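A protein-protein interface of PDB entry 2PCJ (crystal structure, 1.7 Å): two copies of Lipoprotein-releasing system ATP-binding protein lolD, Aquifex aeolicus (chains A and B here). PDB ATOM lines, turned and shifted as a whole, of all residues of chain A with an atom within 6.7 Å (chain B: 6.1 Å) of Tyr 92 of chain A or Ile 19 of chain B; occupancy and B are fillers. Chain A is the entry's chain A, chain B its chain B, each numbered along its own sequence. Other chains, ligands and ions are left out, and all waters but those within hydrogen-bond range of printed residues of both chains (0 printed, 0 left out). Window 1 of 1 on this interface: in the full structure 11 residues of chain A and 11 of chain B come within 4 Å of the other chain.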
ATOM      1  N   PHE A  88       8.289 -16.955 -19.215  1.00  0.00           N
ATOM      2  CA  PHE A  88       8.794 -15.690 -18.695  1.00  0.00           C
ATOM      3  C   PHE A  88      10.301 -15.631 -18.889  1.00  0.00           C
ATOM      4  O   PHE A  88      10.908 -16.574 -19.404  1.00  0.00           O
ATOM      5  CB  PHE A  88       8.472 -15.570 -17.207  1.00  0.00           C
ATOM      6  CG  PHE A  88       7.008 -15.634 -16.899  1.00  0.00           C
ATOM      7  CD1 PHE A  88       6.192 -14.529 -17.110  1.00  0.00           C
ATOM      8  CD2 PHE A  88       6.439 -16.808 -16.423  1.00  0.00           C
ATOM      9  CE1 PHE A  88       4.822 -14.594 -16.847  1.00  0.00           C
ATOM     10  CE2 PHE A  88       5.072 -16.883 -16.159  1.00  0.00           C
ATOM     11  CZ  PHE A  88       4.264 -15.773 -16.373  1.00  0.00           C
ATOM     12  N   GLN A  89      10.909 -14.523 -18.486  1.00  0.00           N
ATOM     13  CA  GLN A  89      12.352 -14.397 -18.625  1.00  0.00           C
ATOM     14  C   GLN A  89      13.016 -15.436 -17.723  1.00  0.00           C
ATOM     15  O   GLN A  89      13.955 -16.116 -18.139  1.00  0.00           O
ATOM     16  CB  GLN A  89      12.821 -12.994 -18.240  1.00  0.00           C
ATOM     17  CG  GLN A  89      14.286 -12.757 -18.594  1.00  0.00           C
ATOM     18  CD  GLN A  89      14.728 -11.320 -18.394  1.00  0.00           C
ATOM     19  OE1 GLN A  89      13.956 -10.385 -18.605  1.00  0.00           O
ATOM     20  NE2 GLN A  89      15.986 -11.136 -18.009  1.00  0.00           N
ATOM     21  N   PHE A  90      12.525 -15.543 -16.489  1.00  0.00           N
ATOM     22  CA  PHE A  90      13.041 -16.523 -15.534  1.00  0.00           C
ATOM     23  C   PHE A  90      12.297 -17.826 -15.820  1.00  0.00           C
ATOM     24  O   PHE A  90      11.124 -17.802 -16.197  1.00  0.00           O
ATOM     25  CB  PHE A  90      12.775 -16.071 -14.093  1.00  0.00           C
ATOM     26  CG  PHE A  90      13.349 -16.994 -13.050  1.00  0.00           C
ATOM     27  CD1 PHE A  90      14.716 -17.257 -13.015  1.00  0.00           C
ATOM     28  CD2 PHE A  90      12.526 -17.587 -12.097  1.00  0.00           C
ATOM     29  CE1 PHE A  90      15.260 -18.099 -12.042  1.00  0.00           C
ATOM     30  CE2 PHE A  90      13.058 -18.433 -11.119  1.00  0.00           C
ATOM     31  CZ  PHE A  90      14.428 -18.687 -11.094  1.00  0.00           C
ATOM     32  N   HIS A  91      12.973 -18.956 -15.634  1.00  0.00           N
ATOM     33  CA  HIS A  91      12.389 -20.267 -15.916  1.00  0.00           C
ATOM     34  C   HIS A  91      11.266 -20.735 -14.987  1.00  0.00           C
ATOM     35  O   HIS A  91      10.403 -21.513 -15.397  1.00  0.00           O
ATOM     36  CB  HIS A  91      13.497 -21.329 -15.947  1.00  0.00           C
ATOM     37  CG  HIS A  91      14.325 -21.384 -14.699  1.00  0.00           C
ATOM     38  ND1 HIS A  91      13.837 -21.857 -13.499  1.00  0.00           N
ATOM     39  CD2 HIS A  91      15.611 -21.027 -14.466  1.00  0.00           C
ATOM     40  CE1 HIS A  91      14.785 -21.791 -12.583  1.00  0.00           C
ATOM     41  NE2 HIS A  91      15.873 -21.291 -13.143  1.00  0.00           N
ATOM     42  N   TYR A  92      11.287 -20.276 -13.740  1.00  0.00           N
ATOM     43  CA  TYR A  92      10.273 -20.662 -12.763  1.00  0.00           C
ATOM     44  C   TYR A  92      10.074 -22.167 -12.623  1.00  0.00           C
ATOM     45  O   TYR A  92       8.950 -22.653 -12.469  1.00  0.00           O
ATOM     46  CB  TYR A  92       8.942 -19.974 -13.084  1.00  0.00           C
ATOM     47  CG  TYR A  92       8.968 -18.499 -12.750  1.00  0.00           C
ATOM     48  CD1 TYR A  92       9.010 -18.075 -11.424  1.00  0.00           C
ATOM     49  CD2 TYR A  92       8.997 -17.532 -13.755  1.00  0.00           C
ATOM     50  CE1 TYR A  92       9.083 -16.725 -11.100  1.00  0.00           C
ATOM     51  CE2 TYR A  92       9.073 -16.172 -13.440  1.00  0.00           C
ATOM     52  CZ  TYR A  92       9.115 -15.780 -12.110  1.00  0.00           C
ATOM     53  OH  TYR A  92       9.192 -14.447 -11.777  1.00  0.00           O
ATOM     54  N   LEU A  93      11.176 -22.903 -12.668  1.00  0.00           N
ATOM     55  CA  LEU A  93      11.129 -24.351 -12.502  1.00  0.00           C
ATOM     56  C   LEU A  93      11.141 -24.646 -11.008  1.00  0.00           C
ATOM     57  O   LEU A  93      11.731 -23.894 -10.229  1.00  0.00           O
ATOM     58  CB  LEU A  93      12.348 -24.998 -13.161  1.00  0.00           C
ATOM     59  CG  LEU A  93      12.439 -24.821 -14.675  1.00  0.00           C
ATOM     60  CD1 LEU A  93      13.741 -25.420 -15.195  1.00  0.00           C
ATOM     61  CD2 LEU A  93      11.246 -25.495 -15.331  1.00  0.00           C
ATOM     62  N   ILE A  94      10.476 -25.722 -10.606  1.00  0.00           N
ATOM     63  CA  ILE A  94      10.451 -26.110  -9.199  1.00  0.00           C
ATOM     64  C   ILE A  94      11.750 -26.885  -8.971  1.00  0.00           C
ATOM     65  O   ILE A  94      11.980 -27.918  -9.593  1.00  0.00           O
ATOM     66  CB  ILE A  94       9.230 -26.996  -8.902  1.00  0.00           C
ATOM     67  CG1 ILE A  94       7.951 -26.212  -9.221  1.00  0.00           C
ATOM     68  CG2 ILE A  94       9.248 -27.441  -7.448  1.00  0.00           C
ATOM     69  CD1 ILE A  94       6.697 -27.055  -9.258  1.00  0.00           C
ATOM     70  N   PRO A  95      12.617 -26.387  -8.073  1.00  0.00           N
ATOM     71  CA  PRO A  95      13.908 -27.017  -7.768  1.00  0.00           C
ATOM     72  C   PRO A  95      13.905 -28.482  -7.344  1.00  0.00           C
ATOM     73  O   PRO A  95      14.833 -29.222  -7.666  1.00  0.00           O
ATOM     74  CB  PRO A  95      14.498 -26.093  -6.698  1.00  0.00           C
ATOM     75  CG  PRO A  95      13.294 -25.544  -6.019  1.00  0.00           C
ATOM     76  CD  PRO A  95      12.365 -25.250  -7.172  1.00  0.00           C
ATOM     77  N   ASN A 102       8.571 -31.356 -13.786  1.00  0.00           N
ATOM     78  CA  ASN A 102       8.215 -29.943 -13.931  1.00  0.00           C
ATOM     79  C   ASN A 102       7.272 -29.735 -15.113  1.00  0.00           C
ATOM     80  O   ASN A 102       6.337 -28.938 -15.044  1.00  0.00           O
ATOM     81  CB  ASN A 102       9.470 -29.087 -14.144  1.00  0.00           C
ATOM     82  CG  ASN A 102       9.990 -28.477 -12.854  1.00  0.00           C
ATOM     83  OD1 ASN A 102       9.370 -27.579 -12.285  1.00  0.00           O
ATOM     84  ND2 ASN A 102      11.134 -28.962 -12.390  1.00  0.00           N
ATOM     85  N   GLN A 147      15.365 -22.873 -19.861  1.00  0.00           N
ATOM     86  CA  GLN A 147      14.329 -22.191 -20.633  1.00  0.00           C
ATOM     87  C   GLN A 147      13.592 -23.182 -21.527  1.00  0.00           C
ATOM     88  O   GLN A 147      12.384 -23.058 -21.723  1.00  0.00           O
ATOM     89  CB  GLN A 147      14.911 -21.062 -21.489  1.00  0.00           C
ATOM     90  CG  GLN A 147      15.076 -19.725 -20.770  1.00  0.00           C
ATOM     91  CD  GLN A 147      13.824 -19.300 -20.017  1.00  0.00           C
ATOM     92  OE1 GLN A 147      13.548 -19.804 -18.930  1.00  0.00           O
ATOM     93  NE2 GLN A 147      13.058 -18.374 -20.598  1.00  0.00           N
ATOM     94  N   ALA A 150      10.982 -24.923 -19.608  1.00  0.00           N
ATOM     95  CA  ALA A 150       9.844 -24.025 -19.410  1.00  0.00           C
ATOM     96  C   ALA A 150       8.957 -23.991 -20.657  1.00  0.00           C
ATOM     97  O   ALA A 150       7.731 -23.880 -20.559  1.00  0.00           O
ATOM     98  CB  ALA A 150      10.336 -22.608 -19.078  1.00  0.00           C
ATOM     99  N   ARG A 153       6.962 -27.145 -20.810  1.00  0.00           N
ATOM    100  CA  ARG A 153       5.874 -27.036 -19.847  1.00  0.00           C
ATOM    101  C   ARG A 153       4.756 -26.158 -20.402  1.00  0.00           C
ATOM    102  O   ARG A 153       3.576 -26.429 -20.193  1.00  0.00           O
ATOM    103  CB  ARG A 153       6.392 -26.437 -18.536  1.00  0.00           C
ATOM    104  CG  ARG A 153       5.336 -26.305 -17.447  1.00  0.00           C
ATOM    105  CD  ARG A 153       5.950 -25.744 -16.171  1.00  0.00           C
ATOM    106  NE  ARG A 153       6.538 -24.429 -16.409  1.00  0.00           N
ATOM    107  CZ  ARG A 153       7.375 -23.817 -15.575  1.00  0.00           C
ATOM    108  NH1 ARG A 153       7.730 -24.399 -14.437  1.00  0.00           N
ATOM    109  NH2 ARG A 153       7.859 -22.624 -15.886  1.00  0.00           N
ATOM    110  N   LYS B  12       7.577 -14.584  -0.173  1.00  0.00           N
ATOM    111  CA  LYS B  12       6.548 -14.067  -1.061  1.00  0.00           C
ATOM    112  C   LYS B  12       6.216 -15.166  -2.037  1.00  0.00           C
ATOM    113  O   LYS B  12       7.092 -15.669  -2.739  1.00  0.00           O
ATOM    114  CB  LYS B  12       7.040 -12.835  -1.822  1.00  0.00           C
ATOM    115  CG  LYS B  12       5.996 -12.228  -2.754  1.00  0.00           C
ATOM    116  CD  LYS B  12       4.749 -11.798  -1.983  1.00  0.00           C
ATOM    117  CE  LYS B  12       3.770 -11.055  -2.878  1.00  0.00           C
ATOM    118  NZ  LYS B  12       2.562 -10.602  -2.129  1.00  0.00           N
ATOM    119  N   VAL B  13       4.948 -15.548  -2.059  1.00  0.00           N
ATOM    120  CA  VAL B  13       4.493 -16.599  -2.949  1.00  0.00           C
ATOM    121  C   VAL B  13       3.526 -16.040  -3.976  1.00  0.00           C
ATOM    122  O   VAL B  13       2.608 -15.286  -3.642  1.00  0.00           O
ATOM    123  CB  VAL B  13       3.799 -17.731  -2.162  1.00  0.00           C
ATOM    124  CG1 VAL B  13       3.345 -18.826  -3.118  1.00  0.00           C
ATOM    125  CG2 VAL B  13       4.755 -18.299  -1.119  1.00  0.00           C
ATOM    126  N   ILE B  14       3.746 -16.400  -5.235  1.00  0.00           N
ATOM    127  CA  ILE B  14       2.878 -15.958  -6.318  1.00  0.00           C
ATOM    128  C   ILE B  14       2.468 -17.192  -7.109  1.00  0.00           C
ATOM    129  O   ILE B  14       3.312 -17.896  -7.668  1.00  0.00           O
ATOM    130  CB  ILE B  14       3.589 -14.955  -7.250  1.00  0.00           C
ATOM    131  CG1 ILE B  14       3.891 -13.663  -6.486  1.00  0.00           C
ATOM    132  CG2 ILE B  14       2.704 -14.652  -8.461  1.00  0.00           C
ATOM    133  CD1 ILE B  14       4.636 -12.621  -7.297  1.00  0.00           C
ATOM    134  N   TYR B  17       4.348 -20.277  -6.315  1.00  0.00           N
ATOM    135  CA  TYR B  17       5.801 -20.260  -6.470  1.00  0.00           C
ATOM    136  C   TYR B  17       6.464 -19.296  -5.492  1.00  0.00           C
ATOM    137  O   TYR B  17       6.061 -18.143  -5.392  1.00  0.00           O
ATOM    138  CB  TYR B  17       6.167 -19.853  -7.899  1.00  0.00           C
ATOM    139  CG  TYR B  17       7.580 -20.211  -8.290  1.00  0.00           C
ATOM    140  CD1 TYR B  17       7.860 -21.424  -8.917  1.00  0.00           C
ATOM    141  CD2 TYR B  17       8.639 -19.347  -8.019  1.00  0.00           C
ATOM    142  CE1 TYR B  17       9.156 -21.767  -9.271  1.00  0.00           C
ATOM    143  CE2 TYR B  17       9.947 -19.682  -8.367  1.00  0.00           C
ATOM    144  CZ  TYR B  17      10.196 -20.895  -8.994  1.00  0.00           C
ATOM    145  OH  TYR B  17      11.481 -21.236  -9.356  1.00  0.00           O
ATOM    146  N   GLU B  18       7.482 -19.766  -4.774  1.00  0.00           N
ATOM    147  CA  GLU B  18       8.168 -18.899  -3.822  1.00  0.00           C
ATOM    148  C   GLU B  18       9.160 -17.964  -4.497  1.00  0.00           C
ATOM    149  O   GLU B  18      10.279 -18.367  -4.822  1.00  0.00           O
ATOM    150  CB  GLU B  18       8.904 -19.726  -2.763  1.00  0.00           C
ATOM    151  CG  GLU B  18       8.000 -20.547  -1.866  1.00  0.00           C
ATOM    152  CD  GLU B  18       8.751 -21.153  -0.691  1.00  0.00           C
ATOM    153  OE1 GLU B  18       8.147 -21.948   0.059  1.00  0.00           O
ATOM    154  OE2 GLU B  18       9.946 -20.832  -0.515  1.00  0.00           O
ATOM    155  N   ILE B  19       8.737 -16.716  -4.701  1.00  0.00           N
ATOM    156  CA  ILE B  19       9.571 -15.683  -5.317  1.00  0.00           C
ATOM    157  C   ILE B  19      10.677 -15.300  -4.334  1.00  0.00           C
ATOM    158  O   ILE B  19      11.821 -15.049  -4.729  1.00  0.00           O
ATOM    159  CB  ILE B  19       8.731 -14.429  -5.657  1.00  0.00           C
ATOM    160  CG1 ILE B  19       7.612 -14.799  -6.637  1.00  0.00           C
ATOM    161  CG2 ILE B  19       9.621 -13.345  -6.252  1.00  0.00           C
ATOM    162  CD1 ILE B  19       8.104 -15.354  -7.965  1.00  0.00           C
ATOM    163  N   LEU B  20      10.316 -15.232  -3.052  1.00  0.00           N
ATOM    164  CA  LEU B  20      11.264 -14.938  -1.976  1.00  0.00           C
ATOM    165  C   LEU B  20      11.103 -16.111  -1.015  1.00  0.00           C
ATOM    166  O   LEU B  20       9.995 -16.392  -0.550  1.00  0.00           O
ATOM    167  CB  LEU B  20      10.927 -13.610  -1.289  1.00  0.00           C
ATOM    168  CG  LEU B  20      11.068 -12.364  -2.172  1.00  0.00           C
ATOM    169  CD1 LEU B  20      10.667 -11.130  -1.369  1.00  0.00           C
ATOM    170  CD2 LEU B  20      12.506 -12.234  -2.683  1.00  0.00           C
ATOM    171  N   LYS B  21      12.209 -16.788  -0.725  1.00  0.00           N
ATOM    172  CA  LYS B  21      12.191 -17.994   0.104  1.00  0.00           C
ATOM    173  C   LYS B  21      12.615 -17.876   1.564  1.00  0.00           C
ATOM    174  O   LYS B  21      12.951 -18.882   2.189  1.00  0.00           O
ATOM    175  CB  LYS B  21      13.052 -19.061  -0.579  1.00  0.00           C
ATOM    176  CG  LYS B  21      12.669 -19.296  -2.032  1.00  0.00           C
ATOM    177  CD  LYS B  21      13.610 -20.258  -2.726  1.00  0.00           C
ATOM    178  CE  LYS B  21      13.140 -20.549  -4.142  1.00  0.00           C
ATOM    179  NZ  LYS B  21      13.011 -19.307  -4.952  1.00  0.00           N
ATOM    180  N   GLY B  40      15.366 -13.810 -11.502  1.00  0.00           N
ATOM    181  CA  GLY B  40      15.078 -14.855 -10.538  1.00  0.00           C
ATOM    182  C   GLY B  40      15.520 -14.506  -9.129  1.00  0.00           C
ATOM    183  O   GLY B  40      15.189 -15.217  -8.177  1.00  0.00           O
ATOM    184  N   SER B  41      16.261 -13.412  -8.979  1.00  0.00           N
ATOM    185  CA  SER B  41      16.738 -13.024  -7.654  1.00  0.00           C
ATOM    186  C   SER B  41      15.598 -12.606  -6.742  1.00  0.00           C
ATOM    187  O   SER B  41      15.634 -12.873  -5.536  1.00  0.00           O
ATOM    188  CB  SER B  41      17.768 -11.886  -7.754  1.00  0.00           C
ATOM    189  OG  SER B  41      17.169 -10.658  -8.128  1.00  0.00           O
ATOM    190  N   GLY B  42      14.592 -11.956  -7.321  1.00  0.00           N
ATOM    191  CA  GLY B  42      13.448 -11.488  -6.552  1.00  0.00           C
ATOM    192  C   GLY B  42      13.735 -10.168  -5.860  1.00  0.00           C
ATOM    193  O   GLY B  42      12.967  -9.726  -5.004  1.00  0.00           O
ATOM    194  N   THR B  45      10.912  -7.566  -6.029  1.00  0.00           N
ATOM    195  CA  THR B  45       9.779  -7.982  -5.218  1.00  0.00           C
ATOM    196  C   THR B  45      10.093  -7.681  -3.760  1.00  0.00           C
ATOM    197  O   THR B  45       9.219  -7.245  -3.008  1.00  0.00           O
ATOM    198  CB  THR B  45       9.494  -9.481  -5.385  1.00  0.00           C
ATOM    199  OG1 THR B  45       9.058  -9.730  -6.731  1.00  0.00           O
ATOM    200  CG2 THR B  45       8.405  -9.926  -4.413  1.00  0.00           C
ATOM    201  N   ASP B 214      17.879 -16.570  -6.823  1.00  0.00           N
ATOM    202  CA  ASP B 214      16.742 -17.462  -6.640  1.00  0.00           C
ATOM    203  C   ASP B 214      15.918 -17.194  -5.377  1.00  0.00           C
ATOM    204  O   ASP B 214      15.576 -18.125  -4.646  1.00  0.00           O
ATOM    205  CB  ASP B 214      17.219 -18.918  -6.641  1.00  0.00           C
ATOM    206  CG  ASP B 214      17.864 -19.323  -7.957  1.00  0.00           C
ATOM    207  OD1 ASP B 214      17.235 -19.121  -9.017  1.00  0.00           O
ATOM    208  OD2 ASP B 214      18.998 -19.848  -7.930  1.00  0.00           O
ATOM    209  N   GLY B 215      15.613 -15.923  -5.124  1.00  0.00           N
ATOM    210  CA  GLY B 215      14.796 -15.562  -3.974  1.00  0.00           C
ATOM    211  C   GLY B 215      15.440 -15.650  -2.603  1.00  0.00           C
ATOM    212  O   GLY B 215      14.740 -15.673  -1.592  1.00  0.00           O
ATOM    213  N   LYS B 216      16.767 -15.680  -2.561  1.00  0.00           N
ATOM    214  CA  LYS B 216      17.483 -15.762  -1.290  1.00  0.00           C
ATOM    215  C   LYS B 216      18.671 -14.817  -1.275  1.00  0.00           C
ATOM    216  O   LYS B 216      19.210 -14.475  -2.327  1.00  0.00           O
ATOM    217  CB  LYS B 216      18.004 -17.186  -1.075  1.00  0.00           C
ATOM    218  CG  LYS B 216      16.932 -18.266  -1.093  1.00  0.00           C
ATOM    219  CD  LYS B 216      17.541 -19.659  -1.213  1.00  0.00           C
ATOM    220  CE  LYS B 216      18.218 -19.859  -2.564  1.00  0.00           C
ATOM    221  NZ  LYS B 216      18.772 -21.235  -2.714  1.00  0.00           N
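Phe 90 of chain A touches Tyr 17 of chain B. CA of Gly 40 of chain B touches CD1 of Phe 90 of chain A (3.5 Å). CZ of Phe 90 of chain A touches OD1 of Asp 214 of chain B, 3.5 Å away. O of Tyr 92 of chain A touches CE1 of Tyr 17 of chain B (3.3 Å). CE1 of Tyr 92 of chain A touches CD1 of Ile 19 of chain B (3.6 Å).
O of Leu 93 of chain A sits at hydrogen-bond distance from OH of Tyr 17 of chain B, at 2.8 Å.
A ring nitrogen (ND1) of His 91 of chain A sits at hydrogen-bond distance from the backbone NH (N) of Leu 93 of chain A (3.0 Å). The backbone carbonyl oxygen (O) of Tyr 92 of chain A lies within hydrogen-bond range of the guanidinium group (NH1) of Arg 153 of chain A (2.9 Å). The backbone carbonyl oxygen of Lys 12 of chain B is in hydrogen-bond range of the backbone NH of Ile 19 of chain B (2.8 Å). The side-chain amino group (NZ) of Lys 21 of chain B is in hydrogen-bond range of the backbone carbonyl oxygen (O) of Asp 214 of chain B (2.8 Å). The backbone NH (N) of Asp 214 of chain B sits close to the backbone carbonyl oxygen (O) of Gly 40 of chain B (3.3 Å). The backbone NH of Gly 215 of chain B sits at hydrogen-bond distance from the backbone carbonyl oxygen of Gly 40 of chain B.
Along chain B the printed residues that touch a printed residue of chain A span positions 17 to 214.
Tyr 92 of chain A touches two residues of chain B. Printed residues of chain A within 4 Å of Ile 19 of chain B: Tyr 92. Of the printed residues of chain A, Asp 214 of chain B touches Phe 90 (3.5 Å). Of the printed residues of chain A, Gly 40 of chain B touches Phe 90. Lys 216 of chain B touches none of the printed residues of chain A. The nearest residue of chain A that does not touch Ile 19 of chain B is Phe 90 of chain A (6.5 Å). The nearest printed residue of chain B that does not touch Leu 93 of chain A is Lys 21 of chain B (7.1 Å).
No position is printed for both chains. Of the 6 pairs that touch across the chains among the printed residues, none has its exchanged pair printed and touching as well.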
